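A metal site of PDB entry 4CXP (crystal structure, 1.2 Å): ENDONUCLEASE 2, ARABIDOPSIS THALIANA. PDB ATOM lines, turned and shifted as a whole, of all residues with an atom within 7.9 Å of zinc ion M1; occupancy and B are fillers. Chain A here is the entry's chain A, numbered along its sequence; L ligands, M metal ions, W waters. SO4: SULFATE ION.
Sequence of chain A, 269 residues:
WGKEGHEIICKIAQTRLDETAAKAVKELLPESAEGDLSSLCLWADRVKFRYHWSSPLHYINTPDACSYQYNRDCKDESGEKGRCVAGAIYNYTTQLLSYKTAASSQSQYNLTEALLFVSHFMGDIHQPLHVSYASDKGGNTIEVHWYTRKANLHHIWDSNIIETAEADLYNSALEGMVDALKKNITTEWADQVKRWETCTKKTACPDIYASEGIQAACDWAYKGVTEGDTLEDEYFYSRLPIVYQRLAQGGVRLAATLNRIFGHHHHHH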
ATOM      1  N   TRP A   1     -23.518   1.178 -20.825  1.00  0.00           N
ATOM      2  CA  TRP A   1     -23.956  -0.232 -20.740  1.00  0.00           C
ATOM      3  C   TRP A   1     -25.241  -0.311 -19.951  1.00  0.00           C
ATOM      4  O   TRP A   1     -25.521   0.563 -19.127  1.00  0.00           O
ATOM      5  CB  TRP A   1     -22.920  -1.098 -20.010  1.00  0.00           C
ATOM      6  CG  TRP A   1     -21.514  -1.026 -20.555  1.00  0.00           C
ATOM      7  CD1 TRP A   1     -20.516  -0.265 -20.065  1.00  0.00           C
ATOM      8  CD2 TRP A   1     -20.963  -1.745 -21.666  1.00  0.00           C
ATOM      9  NE1 TRP A   1     -19.373  -0.461 -20.786  1.00  0.00           N
ATOM     10  CE2 TRP A   1     -19.619  -1.373 -21.778  1.00  0.00           C
ATOM     11  CE3 TRP A   1     -21.479  -2.667 -22.581  1.00  0.00           C
ATOM     12  CZ2 TRP A   1     -18.788  -1.891 -22.756  1.00  0.00           C
ATOM     13  CZ3 TRP A   1     -20.641  -3.179 -23.563  1.00  0.00           C
ATOM     14  CH2 TRP A   1     -19.315  -2.792 -23.636  1.00  0.00           C
ATOM     15  N   GLY A   2     -25.961  -1.406 -20.136  1.00  0.00           N
ATOM     16  CA  GLY A   2     -27.027  -1.787 -19.223  1.00  0.00           C
ATOM     17  C   GLY A   2     -26.499  -2.417 -17.959  1.00  0.00           C
ATOM     18  O   GLY A   2     -25.300  -2.392 -17.650  1.00  0.00           O
ATOM     19  N   HIS A   6     -22.310  -3.013 -16.483  1.00  0.00           N
ATOM     20  CA  HIS A   6     -21.783  -2.313 -15.310  1.00  0.00           C
ATOM     21  C   HIS A   6     -21.462  -3.266 -14.167  1.00  0.00           C
ATOM     22  O   HIS A   6     -20.477  -3.078 -13.457  1.00  0.00           O
ATOM     23  CB  HIS A   6     -22.734  -1.219 -14.840  1.00  0.00           C
ATOM     24  CG  HIS A   6     -22.753  -0.063 -15.769  1.00  0.00           C
ATOM     25  ND1 HIS A   6     -21.710   0.834 -15.867  1.00  0.00           N
ATOM     26  CD2 HIS A   6     -23.643   0.294 -16.724  1.00  0.00           C
ATOM     27  CE1 HIS A   6     -21.986   1.696 -16.838  1.00  0.00           C
ATOM     28  NE2 HIS A   6     -23.147   1.395 -17.378  1.00  0.00           N
ATOM     29  N   ASP A  45     -27.341   5.950 -13.633  1.00  0.00           N
ATOM     30  CA  ASP A  45     -28.436   5.973 -14.609  1.00  0.00           C
ATOM     31  C   ASP A  45     -29.773   6.358 -13.967  1.00  0.00           C
ATOM     32  O   ASP A  45     -30.604   6.950 -14.648  1.00  0.00           O
ATOM     33  CB  ASP A  45     -28.583   4.617 -15.306  1.00  0.00           C
ATOM     34  CG  ASP A  45     -27.671   4.434 -16.477  1.00  0.00           C
ATOM     35  OD1 ASP A  45     -26.963   5.343 -16.910  1.00  0.00           O
ATOM     36  OD2 ASP A  45     -27.680   3.287 -16.974  1.00  0.00           O
ATOM     37  N   LYS A  48     -30.455  10.366 -13.781  1.00  0.00           N
ATOM     38  CA  LYS A  48     -30.442  11.145 -15.021  1.00  0.00           C
ATOM     39  C   LYS A  48     -31.461  12.257 -15.065  1.00  0.00           C
ATOM     40  O   LYS A  48     -31.237  13.254 -15.749  1.00  0.00           O
ATOM     41  CB  LYS A  48     -30.625  10.235 -16.257  1.00  0.00           C
ATOM     42  CG  LYS A  48     -29.372   9.501 -16.660  1.00  0.00           C
ATOM     43  CD  LYS A  48     -29.661   8.552 -17.814  1.00  0.00           C
ATOM     44  CE  LYS A  48     -28.406   7.827 -18.270  1.00  0.00           C
ATOM     45  NZ  LYS A  48     -28.731   6.789 -19.283  1.00  0.00           N
ATOM     46  N   HIS A  58     -22.856  10.904 -19.442  1.00  0.00           N
ATOM     47  CA  HIS A  58     -22.731   9.468 -19.720  1.00  0.00           C
ATOM     48  C   HIS A  58     -22.052   9.166 -21.046  1.00  0.00           C
ATOM     49  O   HIS A  58     -21.713   8.012 -21.295  1.00  0.00           O
ATOM     50  CB  HIS A  58     -24.095   8.789 -19.697  1.00  0.00           C
ATOM     51  CG  HIS A  58     -24.711   8.783 -18.336  1.00  0.00           C
ATOM     52  ND1 HIS A  58     -24.939   7.628 -17.624  1.00  0.00           N
ATOM     53  CD2 HIS A  58     -25.102   9.815 -17.555  1.00  0.00           C
ATOM     54  CE1 HIS A  58     -25.446   7.967 -16.443  1.00  0.00           C
ATOM     55  NE2 HIS A  58     -25.562   9.288 -16.377  1.00  0.00           N
ATOM     56  N   TYR A  59     -21.844  10.167 -21.908  1.00  0.00           N
ATOM     57  CA  TYR A  59     -21.382   9.883 -23.263  1.00  0.00           C
ATOM     58  C   TYR A  59     -20.556  11.035 -23.799  1.00  0.00           C
ATOM     59  O   TYR A  59     -20.377  12.070 -23.151  1.00  0.00           O
ATOM     60  CB  TYR A  59     -22.604   9.550 -24.169  1.00  0.00           C
ATOM     61  CG  TYR A  59     -23.608  10.667 -24.206  1.00  0.00           C
ATOM     62  CD1 TYR A  59     -23.441  11.777 -25.051  1.00  0.00           C
ATOM     63  CD2 TYR A  59     -24.710  10.660 -23.361  1.00  0.00           C
ATOM     64  CE1 TYR A  59     -24.356  12.806 -25.053  1.00  0.00           C
ATOM     65  CE2 TYR A  59     -25.611  11.705 -23.362  1.00  0.00           C
ATOM     66  CZ  TYR A  59     -25.438  12.775 -24.206  1.00  0.00           C
ATOM     67  OH  TYR A  59     -26.344  13.808 -24.187  1.00  0.00           O
ATOM     68  N   HIS A 120     -19.543   4.152 -12.538  1.00  0.00           N
ATOM     69  CA  HIS A 120     -20.427   4.046 -13.688  1.00  0.00           C
ATOM     70  C   HIS A 120     -19.797   4.647 -14.939  1.00  0.00           C
ATOM     71  O   HIS A 120     -19.839   4.047 -16.015  1.00  0.00           O
ATOM     72  CB  HIS A 120     -21.752   4.757 -13.383  1.00  0.00           C
ATOM     73  CG  HIS A 120     -22.764   4.595 -14.462  1.00  0.00           C
ATOM     74  ND1 HIS A 120     -23.662   3.561 -14.492  1.00  0.00           N
ATOM     75  CD2 HIS A 120     -23.043   5.360 -15.549  1.00  0.00           C
ATOM     76  CE1 HIS A 120     -24.426   3.676 -15.566  1.00  0.00           C
ATOM     77  NE2 HIS A 120     -24.086   4.770 -16.214  1.00  0.00           N
ATOM     78  N   ASP A 124     -19.121   3.451 -18.735  1.00  0.00           N
ATOM     79  CA  ASP A 124     -19.728   4.019 -19.930  1.00  0.00           C
ATOM     80  C   ASP A 124     -18.693   4.452 -20.956  1.00  0.00           C
ATOM     81  O   ASP A 124     -18.920   4.303 -22.147  1.00  0.00           O
ATOM     82  CB  ASP A 124     -20.690   5.155 -19.581  1.00  0.00           C
ATOM     83  CG  ASP A 124     -22.110   4.698 -19.290  1.00  0.00           C
ATOM     84  OD1 ASP A 124     -22.345   3.483 -19.380  1.00  0.00           O
ATOM     85  OD2 ASP A 124     -22.926   5.571 -18.988  1.00  0.00           O
ATOM     86  N   GLN A 127     -17.968   1.738 -23.431  1.00  0.00           N
ATOM     87  CA  GLN A 127     -18.973   1.251 -24.378  1.00  0.00           C
ATOM     88  C   GLN A 127     -18.718   2.011 -25.685  1.00  0.00           C
ATOM     89  O   GLN A 127     -18.805   3.237 -25.704  1.00  0.00           O
ATOM     90  CB  GLN A 127     -20.371   1.524 -23.802  1.00  0.00           C
ATOM     91  CG  GLN A 127     -21.484   0.581 -24.238  1.00  0.00           C
ATOM     92  CD  GLN A 127     -21.988   0.791 -25.655  1.00  0.00           C
ATOM     93  OE1 GLN A 127     -21.207   0.711 -26.608  1.00  0.00           O
ATOM     94  NE2 GLN A 127     -23.282   1.030 -25.813  1.00  0.00           N
ATOM     95  N   LEU A 129     -20.296   2.750 -28.352  1.00  0.00           N
ATOM     96  CA  LEU A 129     -21.334   3.681 -28.790  1.00  0.00           C
ATOM     97  C   LEU A 129     -21.685   4.759 -27.793  1.00  0.00           C
ATOM     98  O   LEU A 129     -22.538   5.571 -28.066  1.00  0.00           O
ATOM     99  CB  LEU A 129     -22.562   2.939 -29.308  1.00  0.00           C
ATOM    100  CG  LEU A 129     -22.340   2.178 -30.613  1.00  0.00           C
ATOM    101  CD1 LEU A 129     -23.592   1.435 -31.009  1.00  0.00           C
ATOM    102  CD2 LEU A 129     -21.907   3.085 -31.744  1.00  0.00           C
ATOM    103  N   HIS A 130     -20.987   4.813 -26.654  1.00  0.00           N
ATOM    104  CA  HIS A 130     -20.995   5.998 -25.788  1.00  0.00           C
ATOM    105  C   HIS A 130     -19.959   7.039 -26.202  1.00  0.00           C
ATOM    106  O   HIS A 130     -19.918   8.081 -25.594  1.00  0.00           O
ATOM    107  CB  HIS A 130     -20.819   5.605 -24.323  1.00  0.00           C
ATOM    108  CG  HIS A 130     -22.101   5.164 -23.686  1.00  0.00           C
ATOM    109  ND1 HIS A 130     -22.655   5.793 -22.613  1.00  0.00           N
ATOM    110  CD2 HIS A 130     -22.977   4.181 -24.022  1.00  0.00           C
ATOM    111  CE1 HIS A 130     -23.810   5.232 -22.314  1.00  0.00           C
ATOM    112  NE2 HIS A 130     -24.030   4.243 -23.165  1.00  0.00           N
ATOM    113  N   GLY A 138     -25.496   8.298 -31.038  1.00  0.00           N
ATOM    114  CA  GLY A 138     -24.743   7.156 -30.548  1.00  0.00           C
ATOM    115  C   GLY A 138     -25.331   5.824 -30.950  1.00  0.00           C
ATOM    116  O   GLY A 138     -25.272   4.847 -30.196  1.00  0.00           O
ATOM    117  N   ASN A 140     -28.500   5.240 -31.330  1.00  0.00           N
ATOM    118  CA  ASN A 140     -29.864   5.122 -30.877  1.00  0.00           C
ATOM    119  C   ASN A 140     -30.889   5.240 -32.002  1.00  0.00           C
ATOM    120  O   ASN A 140     -31.968   4.660 -31.888  1.00  0.00           O
ATOM    121  CB  ASN A 140     -30.192   6.125 -29.787  1.00  0.00           C
ATOM    122  CG  ASN A 140     -29.763   5.653 -28.435  1.00  0.00           C
ATOM    123  OD1 ASN A 140     -30.408   4.787 -27.846  1.00  0.00           O
ATOM    124  ND2 ASN A 140     -28.663   6.199 -27.925  1.00  0.00           N
ATOM    125  N   HIS A 154     -27.548   1.096 -30.492  1.00  0.00           N
ATOM    126  CA  HIS A 154     -27.023   1.454 -29.198  1.00  0.00           C
ATOM    127  C   HIS A 154     -27.389   0.417 -28.122  1.00  0.00           C
ATOM    128  O   HIS A 154     -26.542  -0.018 -27.339  1.00  0.00           O
ATOM    129  CB  HIS A 154     -27.478   2.865 -28.793  1.00  0.00           C
ATOM    130  CG  HIS A 154     -26.822   3.329 -27.541  1.00  0.00           C
ATOM    131  ND1 HIS A 154     -25.741   4.169 -27.547  1.00  0.00           N
ATOM    132  CD2 HIS A 154     -27.031   3.004 -26.251  1.00  0.00           C
ATOM    133  CE1 HIS A 154     -25.334   4.368 -26.309  1.00  0.00           C
ATOM    134  NE2 HIS A 154     -26.094   3.646 -25.492  1.00  0.00           N
ATOM    135  N   HIS A 155     -28.663   0.045 -28.110  1.00  0.00           N
ATOM    136  CA  HIS A 155     -29.161  -0.916 -27.153  1.00  0.00           C
ATOM    137  C   HIS A 155     -28.502  -2.287 -27.328  1.00  0.00           C
ATOM    138  O   HIS A 155     -28.269  -3.005 -26.362  1.00  0.00           O
ATOM    139  CB  HIS A 155     -30.690  -1.010 -27.259  1.00  0.00           C
ATOM    140  CG  HIS A 155     -31.322  -1.761 -26.127  1.00  0.00           C
ATOM    141  ND1 HIS A 155     -31.557  -3.124 -26.147  1.00  0.00           N
ATOM    142  CD2 HIS A 155     -31.757  -1.324 -24.931  1.00  0.00           C
ATOM    143  CE1 HIS A 155     -32.143  -3.482 -25.018  1.00  0.00           C
ATOM    144  NE2 HIS A 155     -32.273  -2.419 -24.255  1.00  0.00           N
ATOM    145  N   TRP A 157     -25.449  -2.817 -28.157  1.00  0.00           N
ATOM    146  CA  TRP A 157     -24.181  -2.709 -27.468  1.00  0.00           C
ATOM    147  C   TRP A 157     -24.324  -2.537 -25.964  1.00  0.00           C
ATOM    148  O   TRP A 157     -23.522  -3.092 -25.208  1.00  0.00           O
ATOM    149  CB  TRP A 157     -23.346  -1.618 -28.144  1.00  0.00           C
ATOM    150  CG  TRP A 157     -22.746  -2.121 -29.408  1.00  0.00           C
ATOM    151  CD1 TRP A 157     -23.359  -2.280 -30.630  1.00  0.00           C
ATOM    152  CD2 TRP A 157     -21.435  -2.696 -29.549  1.00  0.00           C
ATOM    153  NE1 TRP A 157     -22.489  -2.884 -31.509  1.00  0.00           N
ATOM    154  CE2 TRP A 157     -21.302  -3.138 -30.870  1.00  0.00           C
ATOM    155  CE3 TRP A 157     -20.355  -2.858 -28.673  1.00  0.00           C
ATOM    156  CZ2 TRP A 157     -20.147  -3.741 -31.335  1.00  0.00           C
ATOM    157  CZ3 TRP A 157     -19.208  -3.426 -29.148  1.00  0.00           C
ATOM    158  CH2 TRP A 157     -19.103  -3.869 -30.466  1.00  0.00           C
ATOM    159  N   ASP A 158     -25.331  -1.800 -25.501  1.00  0.00           N
ATOM    160  CA  ASP A 158     -25.515  -1.677 -24.057  1.00  0.00           C
ATOM    161  C   ASP A 158     -25.890  -3.024 -23.424  1.00  0.00           C
ATOM    162  O   ASP A 158     -25.427  -3.310 -22.311  1.00  0.00           O
ATOM    163  CB  ASP A 158     -26.647  -0.703 -23.710  1.00  0.00           C
ATOM    164  CG  ASP A 158     -26.235   0.755 -23.609  1.00  0.00           C
ATOM    165  OD1 ASP A 158     -25.032   1.089 -23.555  1.00  0.00           O
ATOM    166  OD2 ASP A 158     -27.170   1.600 -23.529  1.00  0.00           O
ATOM    167  N   SER A 159     -26.756  -3.769 -24.101  1.00  0.00           N
ATOM    168  CA  SER A 159     -27.475  -4.862 -23.481  1.00  0.00           C
ATOM    169  C   SER A 159     -27.583  -6.147 -24.297  1.00  0.00           C
ATOM    170  O   SER A 159     -27.371  -7.229 -23.751  1.00  0.00           O
ATOM    171  CB  SER A 159     -28.901  -4.403 -23.127  1.00  0.00           C
ATOM    172  OG  SER A 159     -28.853  -3.399 -22.128  1.00  0.00           O
HETATM  173  S   SO4 L   1     -26.349   3.945 -19.981  1.00  0.00           S
HETATM  174  O1  SO4 L   1     -27.708   3.483 -19.490  1.00  0.00           O
HETATM  175  O2  SO4 L   1     -26.297   5.525 -20.010  1.00  0.00           O
HETATM  176  O3  SO4 L   1     -26.096   3.171 -21.257  1.00  0.00           O
HETATM  177  O4  SO4 L   1     -25.351   3.548 -18.938  1.00  0.00           O
HETATM  178 ZN    ZN M   1     -25.972   3.390 -23.349  1.00  0.00          ZN
HETATM  179 ZN    ZN M   2     -23.947   2.202 -19.040  1.00  0.00          ZN
HETATM  180 ZN    ZN M   3     -24.900   5.498 -18.121  1.00  0.00          ZN
HETATM  181  O   HOH W   1     -27.449   4.853 -23.174  1.00  0.00           O
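ND1 of His 130 sits at hydrogen-bond distance from O of His 58 (2.7 Å). OD1 of Asp 158 sits close to NE2 of Gln 127 (2.9 Å). The backbone carbonyl oxygen of Asp 158 sits at hydrogen-bond distance from the backbone NH of Gly 2. ND1 of His 154 lies within hydrogen-bond range of O of Gly 138.
Three residues have an atom within 4 Å of zinc ion M1: His 130, His 154 and Asp 158.
Water W1 is bound to zinc ion M1 (2.1 Å). Zinc ion M1 is bound by an oxygen (O3) of the ligand, 2.1 Å away. Zinc ion M1 is bound by NE2 of His 130 (2.1 Å). The side-chain carboxylate (OD2) of Asp 158 binds zinc ion M1 (2.2 Å). NE2 of His 154 is bound to zinc ion M1. Zinc ion M1 is bound by OD1 of Asp 158, at 2.5 Å.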
